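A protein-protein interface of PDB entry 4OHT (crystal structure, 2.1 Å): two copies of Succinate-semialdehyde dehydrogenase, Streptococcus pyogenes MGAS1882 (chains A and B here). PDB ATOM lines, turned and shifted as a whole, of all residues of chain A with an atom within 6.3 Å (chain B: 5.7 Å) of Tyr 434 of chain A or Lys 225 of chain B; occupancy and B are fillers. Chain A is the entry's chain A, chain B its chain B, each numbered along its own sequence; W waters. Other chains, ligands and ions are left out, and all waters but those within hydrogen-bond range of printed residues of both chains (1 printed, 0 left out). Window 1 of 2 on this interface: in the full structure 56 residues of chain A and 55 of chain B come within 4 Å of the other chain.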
ATOM      1  N   ALA A 216       7.841  11.895 -36.795  1.00  0.00           N
ATOM      2  CA  ALA A 216       7.243  12.185 -35.487  1.00  0.00           C
ATOM      3  C   ALA A 216       7.926  13.382 -34.826  1.00  0.00           C
ATOM      4  O   ALA A 216       7.276  14.205 -34.171  1.00  0.00           O
ATOM      5  CB  ALA A 216       7.332  10.956 -34.574  1.00  0.00           C
ATOM      6  N   LYS A 225      -0.675  15.935 -34.079  1.00  0.00           N
ATOM      7  CA  LYS A 225      -0.887  14.572 -33.590  1.00  0.00           C
ATOM      8  C   LYS A 225      -0.374  13.568 -34.628  1.00  0.00           C
ATOM      9  O   LYS A 225      -0.425  13.831 -35.831  1.00  0.00           O
ATOM     10  CB  LYS A 225      -2.379  14.335 -33.348  1.00  0.00           C
ATOM     11  CG  LYS A 225      -2.734  13.015 -32.679  1.00  0.00           C
ATOM     12  CD  LYS A 225      -4.257  12.915 -32.543  1.00  0.00           C
ATOM     13  CE  LYS A 225      -4.697  11.787 -31.619  1.00  0.00           C
ATOM     14  NZ  LYS A 225      -4.293  10.435 -32.101  1.00  0.00           N
ATOM     15  N   THR A 226       0.112  12.421 -34.162  1.00  0.00           N
ATOM     16  CA  THR A 226       0.628  11.382 -35.048  1.00  0.00           C
ATOM     17  C   THR A 226       0.197   9.981 -34.628  1.00  0.00           C
ATOM     18  O   THR A 226      -0.257   9.771 -33.502  1.00  0.00           O
ATOM     19  CB  THR A 226       2.177  11.354 -35.059  1.00  0.00           C
ATOM     20  OG1 THR A 226       2.653  11.235 -33.711  1.00  0.00           O
ATOM     21  CG2 THR A 226       2.750  12.614 -35.689  1.00  0.00           C
ATOM     22  N   THR A 227       0.330   9.040 -35.559  1.00  0.00           N
ATOM     23  CA  THR A 227       0.073   7.626 -35.315  1.00  0.00           C
ATOM     24  C   THR A 227       1.202   6.954 -36.096  1.00  0.00           C
ATOM     25  O   THR A 227       1.512   7.356 -37.223  1.00  0.00           O
ATOM     26  CB  THR A 227      -1.297   7.124 -35.853  1.00  0.00           C
ATOM     27  OG1 THR A 227      -1.345   7.271 -37.274  1.00  0.00           O
ATOM     28  CG2 THR A 227      -2.447   7.894 -35.206  1.00  0.00           C
ATOM     29  N   LEU A 228       1.832   5.953 -35.493  1.00  0.00           N
ATOM     30  CA  LEU A 228       2.939   5.267 -36.129  1.00  0.00           C
ATOM     31  C   LEU A 228       2.758   3.757 -36.170  1.00  0.00           C
ATOM     32  O   LEU A 228       2.513   3.123 -35.143  1.00  0.00           O
ATOM     33  CB  LEU A 228       4.247   5.583 -35.387  1.00  0.00           C
ATOM     34  CG  LEU A 228       4.768   7.022 -35.348  1.00  0.00           C
ATOM     35  CD1 LEU A 228       6.032   7.077 -34.490  1.00  0.00           C
ATOM     36  CD2 LEU A 228       5.067   7.503 -36.767  1.00  0.00           C
ATOM     37  N   GLU A 229       2.879   3.195 -37.370  1.00  0.00           N
ATOM     38  CA  GLU A 229       2.784   1.754 -37.597  1.00  0.00           C
ATOM     39  C   GLU A 229       4.171   1.376 -38.115  1.00  0.00           C
ATOM     40  O   GLU A 229       4.490   1.614 -39.286  1.00  0.00           O
ATOM     41  CB  GLU A 229       1.741   1.444 -38.673  1.00  0.00           C
ATOM     42  CG  GLU A 229       0.312   1.823 -38.316  1.00  0.00           C
ATOM     43  CD  GLU A 229      -0.351   0.801 -37.409  1.00  0.00           C
ATOM     44  OE1 GLU A 229       0.238  -0.285 -37.193  1.00  0.00           O
ATOM     45  OE2 GLU A 229      -1.465   1.080 -36.924  1.00  0.00           O
ATOM     46  N   LEU A 230       4.996   0.800 -37.246  1.00  0.00           N
ATOM     47  CA  LEU A 230       6.351   0.443 -37.635  1.00  0.00           C
ATOM     48  C   LEU A 230       6.577  -1.055 -37.810  1.00  0.00           C
ATOM     49  O   LEU A 230       5.629  -1.830 -37.923  1.00  0.00           O
ATOM     50  CB  LEU A 230       7.338   1.027 -36.623  1.00  0.00           C
ATOM     51  CG  LEU A 230       7.112   2.527 -36.378  1.00  0.00           C
ATOM     52  CD1 LEU A 230       8.087   3.040 -35.334  1.00  0.00           C
ATOM     53  CD2 LEU A 230       7.276   3.299 -37.688  1.00  0.00           C
ATOM     54  N   GLY A 428       0.713  -1.711 -32.782  1.00  0.00           N
ATOM     55  CA  GLY A 428       1.508  -2.360 -31.752  1.00  0.00           C
ATOM     56  C   GLY A 428       2.026  -1.423 -30.678  1.00  0.00           C
ATOM     57  O   GLY A 428       1.478  -0.340 -30.472  1.00  0.00           O
ATOM     58  N   ILE A 429       3.091  -1.846 -29.999  1.00  0.00           N
ATOM     59  CA  ILE A 429       3.707  -1.061 -28.931  1.00  0.00           C
ATOM     60  C   ILE A 429       5.224  -1.033 -29.114  1.00  0.00           C
ATOM     61  O   ILE A 429       5.727  -1.503 -30.132  1.00  0.00           O
ATOM     62  CB  ILE A 429       3.364  -1.654 -27.548  1.00  0.00           C
ATOM     63  CG1 ILE A 429       3.785  -3.122 -27.482  1.00  0.00           C
ATOM     64  CG2 ILE A 429       1.859  -1.551 -27.300  1.00  0.00           C
ATOM     65  CD1 ILE A 429       3.530  -3.773 -26.136  1.00  0.00           C
ATOM     66  N   LYS A 430       5.943  -0.482 -28.138  1.00  0.00           N
ATOM     67  CA  LYS A 430       7.404  -0.399 -28.207  1.00  0.00           C
ATOM     68  C   LYS A 430       7.844   0.201 -29.543  1.00  0.00           C
ATOM     69  O   LYS A 430       7.231   1.145 -30.026  1.00  0.00           O
ATOM     70  CB  LYS A 430       8.026  -1.787 -28.030  1.00  0.00           C
ATOM     71  CG  LYS A 430       7.708  -2.460 -26.693  1.00  0.00           C
ATOM     72  CD  LYS A 430       8.466  -3.776 -26.574  1.00  0.00           C
ATOM     73  CE  LYS A 430       8.112  -4.539 -25.309  1.00  0.00           C
ATOM     74  NZ  LYS A 430       8.879  -5.828 -25.219  1.00  0.00           N
ATOM     75  N   SER A 432       7.330  -0.779 -32.400  1.00  0.00           N
ATOM     76  CA  SER A 432       6.384  -1.029 -33.489  1.00  0.00           C
ATOM     77  C   SER A 432       5.476   0.195 -33.635  1.00  0.00           C
ATOM     78  O   SER A 432       4.648   0.270 -34.541  1.00  0.00           O
ATOM     79  CB  SER A 432       5.546  -2.278 -33.213  1.00  0.00           C
ATOM     80  OG  SER A 432       6.361  -3.438 -33.202  1.00  0.00           O
ATOM     81  N   GLY A 433       5.638   1.161 -32.733  1.00  0.00           N
ATOM     82  CA  GLY A 433       4.841   2.377 -32.806  1.00  0.00           C
ATOM     83  C   GLY A 433       3.767   2.545 -31.746  1.00  0.00           C
ATOM     84  O   GLY A 433       3.851   1.968 -30.657  1.00  0.00           O
ATOM     85  N   TYR A 434       2.764   3.356 -32.069  1.00  0.00           N
ATOM     86  CA  TYR A 434       1.641   3.622 -31.174  1.00  0.00           C
ATOM     87  C   TYR A 434       0.446   4.067 -32.009  1.00  0.00           C
ATOM     88  O   TYR A 434       0.603   4.557 -33.129  1.00  0.00           O
ATOM     89  CB  TYR A 434       2.012   4.704 -30.142  1.00  0.00           C
ATOM     90  CG  TYR A 434       2.582   5.978 -30.733  1.00  0.00           C
ATOM     91  CD1 TYR A 434       1.753   6.938 -31.312  1.00  0.00           C
ATOM     92  CD2 TYR A 434       3.956   6.216 -30.724  1.00  0.00           C
ATOM     93  CE1 TYR A 434       2.281   8.106 -31.869  1.00  0.00           C
ATOM     94  CE2 TYR A 434       4.492   7.377 -31.279  1.00  0.00           C
ATOM     95  CZ  TYR A 434       3.651   8.315 -31.850  1.00  0.00           C
ATOM     96  OH  TYR A 434       4.183   9.441 -32.439  1.00  0.00           O
ATOM     97  N   GLY A 435      -0.750   3.901 -31.462  1.00  0.00           N
ATOM     98  CA  GLY A 435      -1.940   4.265 -32.199  1.00  0.00           C
ATOM     99  C   GLY A 435      -2.443   3.024 -32.903  1.00  0.00           C
ATOM    100  O   GLY A 435      -1.779   1.986 -32.874  1.00  0.00           O
ATOM    101  N   ARG A 436      -3.608   3.117 -33.535  1.00  0.00           N
ATOM    102  CA  ARG A 436      -4.190   1.975 -34.230  1.00  0.00           C
ATOM    103  C   ARG A 436      -4.864   2.410 -35.530  1.00  0.00           C
ATOM    104  O   ARG A 436      -5.290   3.557 -35.669  1.00  0.00           O
ATOM    105  CB  ARG A 436      -5.228   1.289 -33.330  1.00  0.00           C
ATOM    106  CG  ARG A 436      -4.668   0.646 -32.054  1.00  0.00           C
ATOM    107  CD  ARG A 436      -4.052  -0.718 -32.348  1.00  0.00           C
ATOM    108  NE  ARG A 436      -3.547  -1.403 -31.154  1.00  0.00           N
ATOM    109  CZ  ARG A 436      -2.415  -1.096 -30.525  1.00  0.00           C
ATOM    110  NH1 ARG A 436      -1.648  -0.101 -30.964  1.00  0.00           N
ATOM    111  NH2 ARG A 436      -2.037  -1.803 -29.465  1.00  0.00           N
ATOM    112  N   VAL B 201       7.406   4.981 -21.570  1.00  0.00           N
ATOM    113  CA  VAL B 201       6.662   4.705 -22.798  1.00  0.00           C
ATOM    114  C   VAL B 201       5.644   5.742 -23.256  1.00  0.00           C
ATOM    115  O   VAL B 201       4.916   5.507 -24.218  1.00  0.00           O
ATOM    116  CB  VAL B 201       5.918   3.351 -22.693  1.00  0.00           C
ATOM    117  CG1 VAL B 201       6.907   2.238 -22.370  1.00  0.00           C
ATOM    118  CG2 VAL B 201       4.830   3.433 -21.627  1.00  0.00           C
ATOM    119  N   GLY B 202       5.577   6.881 -22.579  1.00  0.00           N
ATOM    120  CA  GLY B 202       4.607   7.886 -22.971  1.00  0.00           C
ATOM    121  C   GLY B 202       4.781   9.167 -22.192  1.00  0.00           C
ATOM    122  O   GLY B 202       5.386   9.163 -21.116  1.00  0.00           O
ATOM    123  N   VAL B 203       4.256  10.264 -22.734  1.00  0.00           N
ATOM    124  CA  VAL B 203       4.361  11.559 -22.083  1.00  0.00           C
ATOM    125  C   VAL B 203       3.082  12.367 -22.239  1.00  0.00           C
ATOM    126  O   VAL B 203       2.576  12.524 -23.353  1.00  0.00           O
ATOM    127  CB  VAL B 203       5.512  12.412 -22.678  1.00  0.00           C
ATOM    128  CG1 VAL B 203       5.752  13.639 -21.809  1.00  0.00           C
ATOM    129  CG2 VAL B 203       6.773  11.588 -22.790  1.00  0.00           C
ATOM    130  N   CYS B 204       2.560  12.873 -21.123  1.00  0.00           N
ATOM    131  CA  CYS B 204       1.367  13.710 -21.158  1.00  0.00           C
ATOM    132  C   CYS B 204       1.747  15.052 -20.547  1.00  0.00           C
ATOM    133  O   CYS B 204       2.161  15.126 -19.386  1.00  0.00           O
ATOM    134  CB  CYS B 204       0.210  13.070 -20.382  1.00  0.00           C
ATOM    135  SG  CYS B 204       0.580  12.653 -18.664  1.00  0.00           S
ATOM    136  N   ALA B 219       9.789  13.581 -27.793  1.00  0.00           N
ATOM    137  CA  ALA B 219       9.048  12.321 -27.756  1.00  0.00           C
ATOM    138  C   ALA B 219       8.982  11.693 -29.144  1.00  0.00           C
ATOM    139  O   ALA B 219       9.138  10.481 -29.293  1.00  0.00           O
ATOM    140  CB  ALA B 219       7.639  12.556 -27.218  1.00  0.00           C
ATOM    141  N   GLY B 220       8.755  12.525 -30.161  1.00  0.00           N
ATOM    142  CA  GLY B 220       8.680  12.030 -31.527  1.00  0.00           C
ATOM    143  C   GLY B 220       9.971  11.358 -31.950  1.00  0.00           C
ATOM    144  O   GLY B 220       9.971  10.259 -32.513  1.00  0.00           O
ATOM    145  N   LEU B 223      10.059   7.996 -30.654  1.00  0.00           N
ATOM    146  CA  LEU B 223       8.893   7.168 -30.950  1.00  0.00           C
ATOM    147  C   LEU B 223       7.964   6.993 -29.752  1.00  0.00           C
ATOM    148  O   LEU B 223       7.344   5.941 -29.607  1.00  0.00           O
ATOM    149  CB  LEU B 223       9.349   5.787 -31.427  1.00  0.00           C
ATOM    150  CG  LEU B 223      10.459   5.703 -32.485  1.00  0.00           C
ATOM    151  CD1 LEU B 223      10.735   4.239 -32.792  1.00  0.00           C
ATOM    152  CD2 LEU B 223      10.052   6.436 -33.753  1.00  0.00           C
ATOM    153  N   LYS B 224       7.864   8.005 -28.895  1.00  0.00           N
ATOM    154  CA  LYS B 224       7.001   7.919 -27.715  1.00  0.00           C
ATOM    155  C   LYS B 224       5.670   8.625 -27.960  1.00  0.00           C
ATOM    156  O   LYS B 224       5.639   9.716 -28.517  1.00  0.00           O
ATOM    157  CB  LYS B 224       7.683   8.565 -26.496  1.00  0.00           C
ATOM    158  CG  LYS B 224       9.079   8.038 -26.157  1.00  0.00           C
ATOM    159  CD  LYS B 224       9.059   6.560 -25.792  1.00  0.00           C
ATOM    160  CE  LYS B 224      10.468   5.998 -25.613  1.00  0.00           C
ATOM    161  NZ  LYS B 224      11.181   6.518 -24.408  1.00  0.00           N
ATOM    162  N   LYS B 225       4.573   8.000 -27.542  1.00  0.00           N
ATOM    163  CA  LYS B 225       3.243   8.586 -27.706  1.00  0.00           C
ATOM    164  C   LYS B 225       3.056   9.744 -26.732  1.00  0.00           C
ATOM    165  O   LYS B 225       3.591   9.720 -25.617  1.00  0.00           O
ATOM    166  CB  LYS B 225       2.167   7.535 -27.446  1.00  0.00           C
ATOM    167  CG  LYS B 225       0.742   8.037 -27.636  1.00  0.00           C
ATOM    168  CD  LYS B 225      -0.248   6.892 -27.448  1.00  0.00           C
ATOM    169  CE  LYS B 225      -1.680   7.337 -27.697  1.00  0.00           C
ATOM    170  NZ  LYS B 225      -2.615   6.181 -27.594  1.00  0.00           N
ATOM    171  N   THR B 226       2.290  10.753 -27.146  1.00  0.00           N
ATOM    172  CA  THR B 226       2.047  11.920 -26.305  1.00  0.00           C
ATOM    173  C   THR B 226       0.627  12.471 -26.387  1.00  0.00           C
ATOM    174  O   THR B 226      -0.127  12.165 -27.312  1.00  0.00           O
ATOM    175  CB  THR B 226       2.978  13.097 -26.688  1.00  0.00           C
ATOM    176  OG1 THR B 226       2.654  13.543 -28.011  1.00  0.00           O
ATOM    177  CG2 THR B 226       4.437  12.678 -26.647  1.00  0.00           C
ATOM    178  N   THR B 227       0.277  13.283 -25.394  1.00  0.00           N
ATOM    179  CA  THR B 227      -1.010  13.975 -25.357  1.00  0.00           C
ATOM    180  C   THR B 227      -0.630  15.371 -24.882  1.00  0.00           C
ATOM    181  O   THR B 227       0.213  15.518 -23.988  1.00  0.00           O
ATOM    182  CB  THR B 227      -2.005  13.357 -24.359  1.00  0.00           C
ATOM    183  OG1 THR B 227      -1.475  13.441 -23.032  1.00  0.00           O
ATOM    184  CG2 THR B 227      -2.279  11.913 -24.715  1.00  0.00           C
ATOM    185  N   THR B 444      -7.723   5.670 -21.585  1.00  0.00           N
ATOM    186  CA  THR B 444      -7.024   4.849 -22.568  1.00  0.00           C
ATOM    187  C   THR B 444      -5.860   5.486 -23.326  1.00  0.00           C
ATOM    188  O   THR B 444      -5.294   4.855 -24.216  1.00  0.00           O
ATOM    189  CB  THR B 444      -8.022   4.297 -23.614  1.00  0.00           C
ATOM    190  OG1 THR B 444      -8.682   5.387 -24.264  1.00  0.00           O
ATOM    191  CG2 THR B 444      -9.067   3.417 -22.943  1.00  0.00           C
ATOM    192  N   SER B 445      -5.492   6.717 -22.985  1.00  0.00           N
ATOM    193  CA  SER B 445      -4.387   7.389 -23.676  1.00  0.00           C
ATOM    194  C   SER B 445      -3.100   6.552 -23.764  1.00  0.00           C
ATOM    195  O   SER B 445      -2.444   6.518 -24.803  1.00  0.00           O
ATOM    196  CB  SER B 445      -4.062   8.721 -22.990  1.00  0.00           C
ATOM    197  OG  SER B 445      -5.169   9.602 -23.007  1.00  0.00           O
ATOM    198  N   PHE B 446      -2.734   5.881 -22.677  1.00  0.00           N
ATOM    199  CA  PHE B 446      -1.511   5.084 -22.666  1.00  0.00           C
ATOM    200  C   PHE B 446      -1.776   3.617 -22.351  1.00  0.00           C
ATOM    201  O   PHE B 446      -1.020   2.959 -21.626  1.00  0.00           O
ATOM    202  CB  PHE B 446      -0.517   5.690 -21.668  1.00  0.00           C
ATOM    203  CG  PHE B 446      -0.125   7.100 -22.006  1.00  0.00           C
ATOM    204  CD1 PHE B 446       0.633   7.369 -23.140  1.00  0.00           C
ATOM    205  CD2 PHE B 446      -0.545   8.165 -21.217  1.00  0.00           C
ATOM    206  CE1 PHE B 446       0.970   8.681 -23.486  1.00  0.00           C
ATOM    207  CE2 PHE B 446      -0.216   9.478 -21.555  1.00  0.00           C
ATOM    208  CZ  PHE B 446       0.542   9.735 -22.692  1.00  0.00           C
ATOM    209  N   VAL B 447      -2.864   3.115 -22.916  1.00  0.00           N
ATOM    210  CA  VAL B 447      -3.261   1.729 -22.752  1.00  0.00           C
ATOM    211  C   VAL B 447      -2.942   0.984 -24.043  1.00  0.00           C
ATOM    212  O   VAL B 447      -3.024   1.549 -25.135  1.00  0.00           O
ATOM    213  CB  VAL B 447      -4.782   1.623 -22.489  1.00  0.00           C
ATOM    214  CG1 VAL B 447      -5.280   0.221 -22.797  1.00  0.00           C
ATOM    215  CG2 VAL B 447      -5.084   1.987 -21.052  1.00  0.00           C
HETATM  216  O   HOH W   1      -1.217   3.200 -28.473  1.00  0.00           O
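O of Tyr 434 of chain A sits at hydrogen-bond distance from N of Leu 228 of chain A, at 3.0 Å.
The backbone carbonyl oxygen (O) of Ala 219 of chain B is in hydrogen-bond range of the backbone NH (N) of Lys 224 of chain B (2.8 Å).
The backbone NH of Leu 230 of chain A is in hydrogen-bond range of the backbone carbonyl oxygen of Ser 432 of chain A (2.8 Å).
O of Lys 225 of chain B sits at hydrogen-bond distance from N of Val 203 of chain B, at 3.0 Å.
NZ of Lys 225 of chain B sits at hydrogen-bond distance from O of Ser 445 of chain B.
The side-chain hydroxyl (OH) of Tyr 434 of chain A is in hydrogen-bond range of the side-chain hydroxyl (OG1) of Thr 226 of chain A, 2.7 Å away.
Among the printed residues, merely in contact across the chains: Ala 216 of chain A with Gly 220 of chain B, Leu 230 of chain A with Leu 223 of chain B, Tyr 434 of chain A with Leu 223 of chain B, Tyr 434 of chain A with Lys 224 of chain B and Tyr 434 of chain A with Lys 225 of chain B.
Of the printed residues of chain A, Lys 225 of chain B touches Tyr 434 (3.7 Å).
Of the printed residues of chain B, Leu 230 of chain A touches Leu 223 (3.9 Å).
Of the printed residues of chain B, Ala 216 of chain A touches Gly 220.
Thr 227 of chain B touches none of the printed residues of chain A.
Of the 15 printed residues of chain B, 4 touch a printed residue of chain A.
Printed residues of chain B that touch a printed residue of chain A: Gly 220, Leu 223, Lys 224 and Lys 225.
Hydrophobic or aromatic side chains of chain B within 4 Å of the printed part of chain A: Leu 223.
Of the 15 printed residues of chain A, 3 touch a printed residue of chain B.
Hydrophobic or aromatic side chains of chain A within 4 Å of the printed part of chain B: Ala 216, Leu 230 and Tyr 434.
Among the printed residues, no Asp or Glu carboxylate lies within 4 Å of a Lys or Arg side-chain nitrogen of the other chain.
3 positions are printed for both chains.
Of the 5 pairs that touch across the chains among the printed residues, none has its exchanged pair printed and touching as well.
Water W1 lies within hydrogen-bond range of the backbone NH of Gly 435 of chain A (3.1 Å) and the side-chain amino group of Lys 225 of chain B (3.4 Å).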
